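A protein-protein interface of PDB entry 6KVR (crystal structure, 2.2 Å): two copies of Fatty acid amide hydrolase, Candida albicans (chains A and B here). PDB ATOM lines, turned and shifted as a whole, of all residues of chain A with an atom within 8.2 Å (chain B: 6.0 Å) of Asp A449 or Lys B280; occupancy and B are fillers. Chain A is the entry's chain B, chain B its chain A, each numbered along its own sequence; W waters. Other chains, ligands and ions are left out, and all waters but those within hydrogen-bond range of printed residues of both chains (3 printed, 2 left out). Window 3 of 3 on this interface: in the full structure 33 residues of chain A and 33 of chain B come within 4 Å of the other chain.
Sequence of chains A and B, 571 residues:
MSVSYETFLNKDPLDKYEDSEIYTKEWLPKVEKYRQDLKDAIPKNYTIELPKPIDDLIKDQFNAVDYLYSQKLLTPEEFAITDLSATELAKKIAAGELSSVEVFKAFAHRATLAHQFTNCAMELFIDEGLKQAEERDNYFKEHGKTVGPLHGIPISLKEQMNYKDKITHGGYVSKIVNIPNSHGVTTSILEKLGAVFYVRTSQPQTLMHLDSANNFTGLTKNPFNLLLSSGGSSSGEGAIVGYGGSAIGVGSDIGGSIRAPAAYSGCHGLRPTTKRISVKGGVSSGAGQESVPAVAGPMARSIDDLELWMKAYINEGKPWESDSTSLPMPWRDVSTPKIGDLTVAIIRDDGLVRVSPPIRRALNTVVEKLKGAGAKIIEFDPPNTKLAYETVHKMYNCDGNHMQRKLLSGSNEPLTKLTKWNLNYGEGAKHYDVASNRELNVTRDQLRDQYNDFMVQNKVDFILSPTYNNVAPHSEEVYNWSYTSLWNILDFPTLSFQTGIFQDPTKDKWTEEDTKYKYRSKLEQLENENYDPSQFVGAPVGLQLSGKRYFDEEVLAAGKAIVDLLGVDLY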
ATOM      1  N   VAL A 442     -31.978  14.337 -20.126  1.00  0.00           N
ATOM      2  CA  VAL A 442     -31.517  14.140 -21.501  1.00  0.00           C
ATOM      3  C   VAL A 442     -31.104  15.473 -22.130  1.00  0.00           C
ATOM      4  O   VAL A 442     -30.018  15.592 -22.708  1.00  0.00           O
ATOM      5  CB  VAL A 442     -32.604  13.426 -22.333  1.00  0.00           C
ATOM      6  CG1 VAL A 442     -32.253  13.454 -23.814  1.00  0.00           C
ATOM      7  CG2 VAL A 442     -32.763  11.973 -21.858  1.00  0.00           C
ATOM      8  N   THR A 443     -31.959  16.499 -22.020  1.00  0.00           N
ATOM      9  CA  THR A 443     -31.610  17.817 -22.566  1.00  0.00           C
ATOM     10  C   THR A 443     -30.343  18.389 -21.934  1.00  0.00           C
ATOM     11  O   THR A 443     -29.489  18.934 -22.638  1.00  0.00           O
ATOM     12  CB  THR A 443     -32.762  18.787 -22.364  1.00  0.00           C
ATOM     13  OG1 THR A 443     -33.942  18.217 -22.937  1.00  0.00           O
ATOM     14  CG2 THR A 443     -32.447  20.126 -23.031  1.00  0.00           C
ATOM     15  N   ARG A 444     -30.218  18.285 -20.609  1.00  0.00           N
ATOM     16  CA  ARG A 444     -28.993  18.705 -19.924  1.00  0.00           C
ATOM     17  C   ARG A 444     -27.752  18.062 -20.538  1.00  0.00           C
ATOM     18  O   ARG A 444     -26.727  18.727 -20.737  1.00  0.00           O
ATOM     19  CB  ARG A 444     -29.079  18.350 -18.439  1.00  0.00           C
ATOM     20  CG  ARG A 444     -27.815  18.658 -17.647  1.00  0.00           C
ATOM     21  CD  ARG A 444     -27.773  17.885 -16.326  1.00  0.00           C
ATOM     22  NE  ARG A 444     -27.660  16.458 -16.588  1.00  0.00           N
ATOM     23  CZ  ARG A 444     -27.895  15.501 -15.704  1.00  0.00           C
ATOM     24  NH1 ARG A 444     -28.261  15.776 -14.462  1.00  0.00           N
ATOM     25  NH2 ARG A 444     -27.751  14.232 -16.071  1.00  0.00           N
ATOM     26  N   ASP A 445     -27.819  16.762 -20.837  1.00  0.00           N
ATOM     27  CA  ASP A 445     -26.632  16.076 -21.339  1.00  0.00           C
ATOM     28  C   ASP A 445     -26.341  16.438 -22.793  1.00  0.00           C
ATOM     29  O   ASP A 445     -25.168  16.505 -23.179  1.00  0.00           O
ATOM     30  CB  ASP A 445     -26.784  14.566 -21.153  1.00  0.00           C
ATOM     31  CG  ASP A 445     -26.674  14.144 -19.667  1.00  0.00           C
ATOM     32  OD1 ASP A 445     -26.268  14.966 -18.803  1.00  0.00           O
ATOM     33  OD2 ASP A 445     -27.051  13.000 -19.349  1.00  0.00           O
ATOM     34  N   GLN A 446     -27.372  16.724 -23.597  1.00  0.00           N
ATOM     35  CA  GLN A 446     -27.121  17.247 -24.938  1.00  0.00           C
ATOM     36  C   GLN A 446     -26.437  18.610 -24.878  1.00  0.00           C
ATOM     37  O   GLN A 446     -25.504  18.876 -25.645  1.00  0.00           O
ATOM     38  CB  GLN A 446     -28.423  17.319 -25.741  1.00  0.00           C
ATOM     39  CG  GLN A 446     -28.873  15.935 -26.217  1.00  0.00           C
ATOM     40  CD  GLN A 446     -30.342  15.864 -26.592  1.00  0.00           C
ATOM     41  OE1 GLN A 446     -31.129  16.764 -26.285  1.00  0.00           O
ATOM     42  NE2 GLN A 446     -30.721  14.778 -27.255  1.00  0.00           N
ATOM     43  N   LEU A 447     -26.861  19.473 -23.952  1.00  0.00           N
ATOM     44  CA  LEU A 447     -26.241  20.788 -23.841  1.00  0.00           C
ATOM     45  C   LEU A 447     -24.786  20.671 -23.403  1.00  0.00           C
ATOM     46  O   LEU A 447     -23.915  21.366 -23.938  1.00  0.00           O
ATOM     47  CB  LEU A 447     -27.025  21.665 -22.857  1.00  0.00           C
ATOM     48  CG  LEU A 447     -28.447  22.003 -23.294  1.00  0.00           C
ATOM     49  CD1 LEU A 447     -29.254  22.569 -22.126  1.00  0.00           C
ATOM     50  CD2 LEU A 447     -28.396  22.992 -24.442  1.00  0.00           C
ATOM     51  N   ARG A 448     -24.513  19.818 -22.416  1.00  0.00           N
ATOM     52  CA  ARG A 448     -23.142  19.647 -21.941  1.00  0.00           C
ATOM     53  C   ARG A 448     -22.222  19.205 -23.065  1.00  0.00           C
ATOM     54  O   ARG A 448     -21.128  19.752 -23.245  1.00  0.00           O
ATOM     55  CB  ARG A 448     -23.102  18.643 -20.797  1.00  0.00           C
ATOM     56  CG  ARG A 448     -23.569  19.226 -19.490  1.00  0.00           C
ATOM     57  CD  ARG A 448     -23.500  18.201 -18.379  1.00  0.00           C
ATOM     58  NE  ARG A 448     -24.184  18.715 -17.204  1.00  0.00           N
ATOM     59  CZ  ARG A 448     -24.228  18.097 -16.035  1.00  0.00           C
ATOM     60  NH1 ARG A 448     -23.698  16.898 -15.869  1.00  0.00           N
ATOM     61  NH2 ARG A 448     -24.803  18.708 -15.002  1.00  0.00           N
ATOM     62  N   ASP A 449     -22.668  18.234 -23.849  1.00  0.00           N
ATOM     63  CA  ASP A 449     -21.873  17.731 -24.953  1.00  0.00           C
ATOM     64  C   ASP A 449     -21.655  18.799 -26.023  1.00  0.00           C
ATOM     65  O   ASP A 449     -20.559  18.906 -26.594  1.00  0.00           O
ATOM     66  CB  ASP A 449     -22.577  16.510 -25.511  1.00  0.00           C
ATOM     67  CG  ASP A 449     -22.101  15.227 -24.848  1.00  0.00           C
ATOM     68  OD1 ASP A 449     -20.976  15.214 -24.272  1.00  0.00           O
ATOM     69  OD2 ASP A 449     -22.899  14.262 -24.833  1.00  0.00           O
ATOM     70  N   GLN A 450     -22.675  19.615 -26.291  1.00  0.00           N
ATOM     71  CA  GLN A 450     -22.530  20.691 -27.266  1.00  0.00           C
ATOM     72  C   GLN A 450     -21.446  21.693 -26.843  1.00  0.00           C
ATOM     73  O   GLN A 450     -20.600  22.092 -27.654  1.00  0.00           O
ATOM     74  CB  GLN A 450     -23.875  21.391 -27.458  1.00  0.00           C
ATOM     75  CG  GLN A 450     -23.819  22.531 -28.444  1.00  0.00           C
ATOM     76  CD  GLN A 450     -25.201  23.050 -28.804  1.00  0.00           C
ATOM     77  OE1 GLN A 450     -26.134  22.986 -28.000  1.00  0.00           O
ATOM     78  NE2 GLN A 450     -25.346  23.533 -30.030  1.00  0.00           N
ATOM     79  N   TYR A 451     -21.450  22.112 -25.571  1.00  0.00           N
ATOM     80  CA  TYR A 451     -20.445  23.081 -25.140  1.00  0.00           C
ATOM     81  C   TYR A 451     -19.084  22.418 -24.946  1.00  0.00           C
ATOM     82  O   TYR A 451     -18.045  23.028 -25.241  1.00  0.00           O
ATOM     83  CB  TYR A 451     -20.891  23.786 -23.855  1.00  0.00           C
ATOM     84  CG  TYR A 451     -21.865  24.931 -24.084  1.00  0.00           C
ATOM     85  CD1 TYR A 451     -23.156  24.687 -24.532  1.00  0.00           C
ATOM     86  CD2 TYR A 451     -21.496  26.247 -23.839  1.00  0.00           C
ATOM     87  CE1 TYR A 451     -24.051  25.707 -24.741  1.00  0.00           C
ATOM     88  CE2 TYR A 451     -22.385  27.288 -24.043  1.00  0.00           C
ATOM     89  CZ  TYR A 451     -23.660  27.010 -24.498  1.00  0.00           C
ATOM     90  OH  TYR A 451     -24.549  28.036 -24.702  1.00  0.00           O
ATOM     91  N   ASN A 452     -19.068  21.172 -24.459  1.00  0.00           N
ATOM     92  CA  ASN A 452     -17.814  20.426 -24.399  1.00  0.00           C
ATOM     93  C   ASN A 452     -17.214  20.261 -25.786  1.00  0.00           C
ATOM     94  O   ASN A 452     -15.999  20.412 -25.966  1.00  0.00           O
ATOM     95  CB  ASN A 452     -18.029  19.055 -23.763  1.00  0.00           C
ATOM     96  CG  ASN A 452     -16.720  18.347 -23.450  1.00  0.00           C
ATOM     97  OD1 ASN A 452     -15.824  18.925 -22.838  1.00  0.00           O
ATOM     98  ND2 ASN A 452     -16.600  17.091 -23.881  1.00  0.00           N
ATOM     99  N   ASP A 453     -18.057  19.940 -26.778  1.00  0.00           N
ATOM    100  CA  ASP A 453     -17.566  19.770 -28.143  1.00  0.00           C
ATOM    101  C   ASP A 453     -17.016  21.079 -28.686  1.00  0.00           C
ATOM    102  O   ASP A 453     -15.999  21.089 -29.387  1.00  0.00           O
ATOM    103  CB  ASP A 453     -18.672  19.248 -29.073  1.00  0.00           C
ATOM    104  CG  ASP A 453     -18.969  17.767 -28.880  1.00  0.00           C
ATOM    105  OD1 ASP A 453     -18.172  17.079 -28.203  1.00  0.00           O
ATOM    106  OD2 ASP A 453     -20.009  17.296 -29.405  1.00  0.00           O
ATOM    107  N   PHE A 454     -17.681  22.195 -28.376  1.00  0.00           N
ATOM    108  CA  PHE A 454     -17.174  23.498 -28.792  1.00  0.00           C
ATOM    109  C   PHE A 454     -15.754  23.714 -28.289  1.00  0.00           C
ATOM    110  O   PHE A 454     -14.857  24.087 -29.053  1.00  0.00           O
ATOM    111  CB  PHE A 454     -18.080  24.615 -28.277  1.00  0.00           C
ATOM    112  CG  PHE A 454     -17.560  25.986 -28.599  1.00  0.00           C
ATOM    113  CD1 PHE A 454     -17.702  26.508 -29.876  1.00  0.00           C
ATOM    114  CD2 PHE A 454     -16.882  26.734 -27.643  1.00  0.00           C
ATOM    115  CE1 PHE A 454     -17.203  27.765 -30.193  1.00  0.00           C
ATOM    116  CE2 PHE A 454     -16.377  28.000 -27.945  1.00  0.00           C
ATOM    117  CZ  PHE A 454     -16.535  28.515 -29.229  1.00  0.00           C
ATOM    118  N   MET A 455     -15.535  23.492 -27.000  1.00  0.00           N
ATOM    119  CA  MET A 455     -14.251  23.788 -26.375  1.00  0.00           C
ATOM    120  C   MET A 455     -13.161  22.848 -26.859  1.00  0.00           C
ATOM    121  O   MET A 455     -12.036  23.276 -27.115  1.00  0.00           O
ATOM    122  CB  MET A 455     -14.401  23.742 -24.852  1.00  0.00           C
ATOM    123  CG  MET A 455     -15.229  24.949 -24.319  1.00  0.00           C
ATOM    124  SD  MET A 455     -15.343  25.042 -22.387  1.00  0.00           S
ATOM    125  CE  MET A 455     -13.669  26.012 -22.073  1.00  0.00           C
ATOM    126  N   VAL A 456     -13.511  21.570 -27.020  1.00  0.00           N
ATOM    127  CA  VAL A 456     -12.535  20.582 -27.470  1.00  0.00           C
ATOM    128  C   VAL A 456     -12.184  20.795 -28.945  1.00  0.00           C
ATOM    129  O   VAL A 456     -11.006  20.851 -29.311  1.00  0.00           O
ATOM    130  CB  VAL A 456     -13.053  19.157 -27.215  1.00  0.00           C
ATOM    131  CG1 VAL A 456     -12.136  18.131 -27.912  1.00  0.00           C
ATOM    132  CG2 VAL A 456     -13.148  18.886 -25.711  1.00  0.00           C
ATOM    133  N   GLN A 457     -13.196  20.921 -29.810  1.00  0.00           N
ATOM    134  CA  GLN A 457     -12.934  21.000 -31.248  1.00  0.00           C
ATOM    135  C   GLN A 457     -12.200  22.281 -31.643  1.00  0.00           C
ATOM    136  O   GLN A 457     -11.460  22.277 -32.634  1.00  0.00           O
ATOM    137  CB  GLN A 457     -14.240  20.872 -32.043  1.00  0.00           C
ATOM    138  CG  GLN A 457     -14.997  19.540 -31.797  1.00  0.00           C
ATOM    139  CD  GLN A 457     -16.437  19.526 -32.350  1.00  0.00           C
ATOM    140  OE1 GLN A 457     -17.044  20.577 -32.593  1.00  0.00           O
ATOM    141  NE2 GLN A 457     -16.987  18.325 -32.533  1.00  0.00           N
ATOM    142  N   LEU A 490     -24.791  23.259 -17.219  1.00  0.00           N
ATOM    143  CA  LEU A 490     -23.620  22.643 -17.835  1.00  0.00           C
ATOM    144  C   LEU A 490     -22.650  22.063 -16.808  1.00  0.00           C
ATOM    145  O   LEU A 490     -21.858  21.174 -17.158  1.00  0.00           O
ATOM    146  CB  LEU A 490     -22.867  23.640 -18.714  1.00  0.00           C
ATOM    147  CG  LEU A 490     -23.599  24.337 -19.865  1.00  0.00           C
ATOM    148  CD1 LEU A 490     -22.653  25.293 -20.552  1.00  0.00           C
ATOM    149  CD2 LEU A 490     -24.165  23.351 -20.873  1.00  0.00           C
ATOM    150  N   PHE A 492     -19.959  23.484 -15.368  1.00  0.00           N
ATOM    151  CA  PHE A 492     -18.577  23.805 -15.671  1.00  0.00           C
ATOM    152  C   PHE A 492     -17.994  24.573 -14.496  1.00  0.00           C
ATOM    153  O   PHE A 492     -18.674  25.444 -13.930  1.00  0.00           O
ATOM    154  CB  PHE A 492     -18.459  24.658 -16.945  1.00  0.00           C
ATOM    155  CG  PHE A 492     -18.652  23.890 -18.252  1.00  0.00           C
ATOM    156  CD1 PHE A 492     -19.310  22.662 -18.287  1.00  0.00           C
ATOM    157  CD2 PHE A 492     -18.166  24.409 -19.450  1.00  0.00           C
ATOM    158  CE1 PHE A 492     -19.489  21.969 -19.497  1.00  0.00           C
ATOM    159  CE2 PHE A 492     -18.316  23.707 -20.662  1.00  0.00           C
ATOM    160  CZ  PHE A 492     -18.994  22.490 -20.681  1.00  0.00           C
ATOM    161  N   ARG A 549     -15.213  20.682 -17.576  1.00  0.00           N
ATOM    162  CA  ARG A 549     -15.569  19.963 -16.353  1.00  0.00           C
ATOM    163  C   ARG A 549     -14.351  19.259 -15.751  1.00  0.00           C
ATOM    164  O   ARG A 549     -13.575  18.606 -16.461  1.00  0.00           O
ATOM    165  CB  ARG A 549     -16.689  18.945 -16.636  1.00  0.00           C
ATOM    166  CG  ARG A 549     -17.965  19.542 -17.221  1.00  0.00           C
ATOM    167  CD  ARG A 549     -19.112  18.533 -17.260  1.00  0.00           C
ATOM    168  NE  ARG A 549     -19.670  18.298 -15.931  1.00  0.00           N
ATOM    169  CZ  ARG A 549     -19.886  17.100 -15.419  1.00  0.00           C
ATOM    170  NH1 ARG A 549     -19.609  15.995 -16.102  1.00  0.00           N
ATOM    171  NH2 ARG A 549     -20.389  17.002 -14.193  1.00  0.00           N
ATOM    172  N   ASN B 162     -24.251   1.404 -30.258  1.00  0.00           N
ATOM    173  CA  ASN B 162     -24.229   1.912 -31.628  1.00  0.00           C
ATOM    174  C   ASN B 162     -23.013   1.383 -32.373  1.00  0.00           C
ATOM    175  O   ASN B 162     -21.877   1.539 -31.920  1.00  0.00           O
ATOM    176  CB  ASN B 162     -24.183   3.452 -31.650  1.00  0.00           C
ATOM    177  CG  ASN B 162     -25.537   4.088 -31.426  1.00  0.00           C
ATOM    178  OD1 ASN B 162     -26.557   3.402 -31.399  1.00  0.00           O
ATOM    179  ND2 ASN B 162     -25.554   5.415 -31.279  1.00  0.00           N
ATOM    180  N   GLY B 184     -20.900   4.308 -31.132  1.00  0.00           N
ATOM    181  CA  GLY B 184     -21.003   4.942 -29.841  1.00  0.00           C
ATOM    182  C   GLY B 184     -19.628   5.307 -29.329  1.00  0.00           C
ATOM    183  O   GLY B 184     -18.604   4.950 -29.921  1.00  0.00           O
ATOM    184  N   VAL B 185     -19.594   6.017 -28.196  1.00  0.00           N
ATOM    185  CA  VAL B 185     -18.318   6.550 -27.715  1.00  0.00           C
ATOM    186  C   VAL B 185     -17.339   5.416 -27.422  1.00  0.00           C
ATOM    187  O   VAL B 185     -16.172   5.460 -27.828  1.00  0.00           O
ATOM    188  CB  VAL B 185     -18.521   7.447 -26.482  1.00  0.00           C
ATOM    189  CG1 VAL B 185     -17.184   7.859 -25.929  1.00  0.00           C
ATOM    190  CG2 VAL B 185     -19.332   8.692 -26.857  1.00  0.00           C
ATOM    191  N   THR B 186     -17.792   4.385 -26.713  1.00  0.00           N
ATOM    192  CA  THR B 186     -16.860   3.345 -26.298  1.00  0.00           C
ATOM    193  C   THR B 186     -16.319   2.576 -27.506  1.00  0.00           C
ATOM    194  O   THR B 186     -15.114   2.308 -27.594  1.00  0.00           O
ATOM    195  CB  THR B 186     -17.536   2.420 -25.282  1.00  0.00           C
ATOM    196  OG1 THR B 186     -17.516   3.059 -24.006  1.00  0.00           O
ATOM    197  CG2 THR B 186     -16.792   1.069 -25.169  1.00  0.00           C
ATOM    198  N   SER B 278     -17.603   5.388 -20.844  1.00  0.00           N
ATOM    199  CA  SER B 278     -18.805   5.974 -21.437  1.00  0.00           C
ATOM    200  C   SER B 278     -19.864   4.929 -21.805  1.00  0.00           C
ATOM    201  O   SER B 278     -19.552   3.858 -22.340  1.00  0.00           O
ATOM    202  CB  SER B 278     -18.446   6.764 -22.689  1.00  0.00           C
ATOM    203  OG  SER B 278     -19.618   7.338 -23.251  1.00  0.00           O
ATOM    204  N   VAL B 279     -21.132   5.264 -21.535  1.00  0.00           N
ATOM    205  CA  VAL B 279     -22.272   4.516 -22.061  1.00  0.00           C
ATOM    206  C   VAL B 279     -23.000   5.294 -23.148  1.00  0.00           C
ATOM    207  O   VAL B 279     -24.058   4.861 -23.605  1.00  0.00           O
ATOM    208  CB  VAL B 279     -23.260   4.094 -20.955  1.00  0.00           C
ATOM    209  CG1 VAL B 279     -22.582   3.176 -19.938  1.00  0.00           C
ATOM    210  CG2 VAL B 279     -23.854   5.314 -20.266  1.00  0.00           C
ATOM    211  N   LYS B 280     -22.454   6.427 -23.583  1.00  0.00           N
ATOM    212  CA  LYS B 280     -23.105   7.235 -24.608  1.00  0.00           C
ATOM    213  C   LYS B 280     -23.149   6.516 -25.960  1.00  0.00           C
ATOM    214  O   LYS B 280     -22.139   5.990 -26.435  1.00  0.00           O
ATOM    215  CB  LYS B 280     -22.382   8.581 -24.741  1.00  0.00           C
ATOM    216  CG  LYS B 280     -22.960   9.482 -25.808  1.00  0.00           C
ATOM    217  CD  LYS B 280     -22.186  10.791 -25.935  1.00  0.00           C
ATOM    218  CE  LYS B 280     -22.633  11.577 -27.168  1.00  0.00           C
ATOM    219  NZ  LYS B 280     -21.924  12.883 -27.165  1.00  0.00           N
ATOM    220  N   GLY B 281     -24.323   6.501 -26.588  1.00  0.00           N
ATOM    221  CA  GLY B 281     -24.441   5.995 -27.944  1.00  0.00           C
ATOM    222  C   GLY B 281     -24.882   4.545 -28.044  1.00  0.00           C
ATOM    223  O   GLY B 281     -24.090   3.674 -28.402  1.00  0.00           O
ATOM    224  N   GLY B 282     -26.138   4.277 -27.719  1.00  0.00           N
ATOM    225  CA  GLY B 282     -26.680   2.931 -27.778  1.00  0.00           C
ATOM    226  C   GLY B 282     -28.185   2.983 -27.625  1.00  0.00           C
ATOM    227  O   GLY B 282     -28.784   4.060 -27.532  1.00  0.00           O
ATOM    228  N   SER B 322     -14.974  13.363 -25.572  1.00  0.00           N
ATOM    229  CA  SER B 322     -16.153  13.261 -26.427  1.00  0.00           C
ATOM    230  C   SER B 322     -17.442  12.953 -25.672  1.00  0.00           C
ATOM    231  O   SER B 322     -18.518  13.018 -26.279  1.00  0.00           O
ATOM    232  CB  SER B 322     -15.942  12.200 -27.529  1.00  0.00           C
ATOM    233  OG  SER B 322     -15.200  11.081 -27.074  1.00  0.00           O
ATOM    234  N   ASP B 323     -17.371  12.644 -24.383  1.00  0.00           N
ATOM    235  CA  ASP B 323     -18.537  12.377 -23.547  1.00  0.00           C
ATOM    236  C   ASP B 323     -18.356  13.185 -22.273  1.00  0.00           C
ATOM    237  O   ASP B 323     -17.493  12.868 -21.443  1.00  0.00           O
ATOM    238  CB  ASP B 323     -18.675  10.884 -23.250  1.00  0.00           C
ATOM    239  CG  ASP B 323     -19.745  10.567 -22.203  1.00  0.00           C
ATOM    240  OD1 ASP B 323     -20.552  11.459 -21.827  1.00  0.00           O
ATOM    241  OD2 ASP B 323     -19.785   9.385 -21.766  1.00  0.00           O
ATOM    242  N   SER B 324     -19.179  14.227 -22.127  1.00  0.00           N
ATOM    243  CA  SER B 324     -19.028  15.163 -21.023  1.00  0.00           C
ATOM    244  C   SER B 324     -19.296  14.505 -19.671  1.00  0.00           C
ATOM    245  O   SER B 324     -18.768  14.962 -18.651  1.00  0.00           O
ATOM    246  CB  SER B 324     -19.971  16.346 -21.235  1.00  0.00           C
ATOM    247  OG  SER B 324     -19.735  17.322 -20.243  1.00  0.00           O
ATOM    248  N   THR B 325     -20.113  13.441 -19.641  1.00  0.00           N
ATOM    249  CA  THR B 325     -20.385  12.706 -18.405  1.00  0.00           C
ATOM    250  C   THR B 325     -19.151  11.964 -17.894  1.00  0.00           C
ATOM    251  O   THR B 325     -19.033  11.713 -16.685  1.00  0.00           O
ATOM    252  CB  THR B 325     -21.519  11.704 -18.646  1.00  0.00           C
ATOM    253  OG1 THR B 325     -22.678  12.396 -19.121  1.00  0.00           O
ATOM    254  CG2 THR B 325     -21.871  10.943 -17.369  1.00  0.00           C
HETATM  255  O   HOH W   1     -20.365  13.395 -15.000  1.00  0.00           O
HETATM  256  O   HOH W   2     -22.905  14.950 -21.025  1.00  0.00           O
HETATM  257  O   HOH W   3     -22.972  12.540 -22.589  1.00  0.00           O
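Printed residues of chain A that touch a printed residue of chain B: Arg A448, Asp A449 and Arg A549.
Among the printed residues, 6 pairs touch across the chains.
Among the printed residues, merely in contact across the chains: Arg A448 with Ser B324, Asp A449 with Ser B322 and Asp A449 with Asp B323.
Asp A449 touches four residues of chain B.
Phe A492 touches none of the printed residues of chain B.
Asn B162 touches none of the printed residues of chain A.
Of the printed residues of chain A, Lys B280 touches Asp A449.
Printed residues of chain A within 4 Å of Ser B322: Asp A449 (3.9 Å).
Of the printed residues of chain A, Ser B324 touches Arg A448 (3.7 Å), Asp A449 (3.0 Å) and Arg A549 (2.9 Å).
The nearest residue of chain B that does not touch Asp A449 is Thr B325 (5.0 Å).
The nearest printed residue of chain B that does not touch Arg A448 is Thr B325 (5.6 Å).
The side-chain amino group (NZ) of Lys B280 lies within salt-bridge range of the side-chain carboxylate (OD2) of Asp A449, at 2.9 Å.
The backbone NH (N) of Ser B324 is in hydrogen-bond range of the side-chain carboxylate (OD1) of Asp A449 (3.0 Å).
The guanidinium group (NH1) of Arg A549 sits at hydrogen-bond distance from the backbone carbonyl oxygen (O) of Ser B324, at 2.9 Å.
Water W1 bridges the backbone carbonyl oxygen (O) of Thr B325 (2.7 Å) and the guanidinium group (NH1) of Arg A549 (2.9 Å).
Water W3 lies within hydrogen-bond range of OD1 of Asp B323 (2.8 Å), OD2 of Asp A449 (2.8 Å) and OG1 of Thr B325 (3.5 Å).
Water W2 bridges OG1 of Thr B325 (3.2 Å) and O of Asp A445 (3.5 Å).
No position is printed for both chains.
Of the 6 pairs that touch across the chains among the printed residues, none has its exchanged pair printed and touching as well.
N of Val B185 lies within hydrogen-bond range of O of Lys B280.
OG of Ser B278 is in hydrogen-bond range of N of Lys B280.
The side-chain carboxylate (OD2) of Asp B323 is in hydrogen-bond range of the side-chain hydroxyl (OG) of Ser B278 (2.5 Å).
The side-chain carboxylate of Asp B323 is in hydrogen-bond range of the backbone NH of Thr B325, at 3.0 Å.
The backbone carbonyl oxygen (O) of Leu A490 sits at hydrogen-bond distance from the guanidinium group (NE) of Arg A448, at 3.4 Å.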
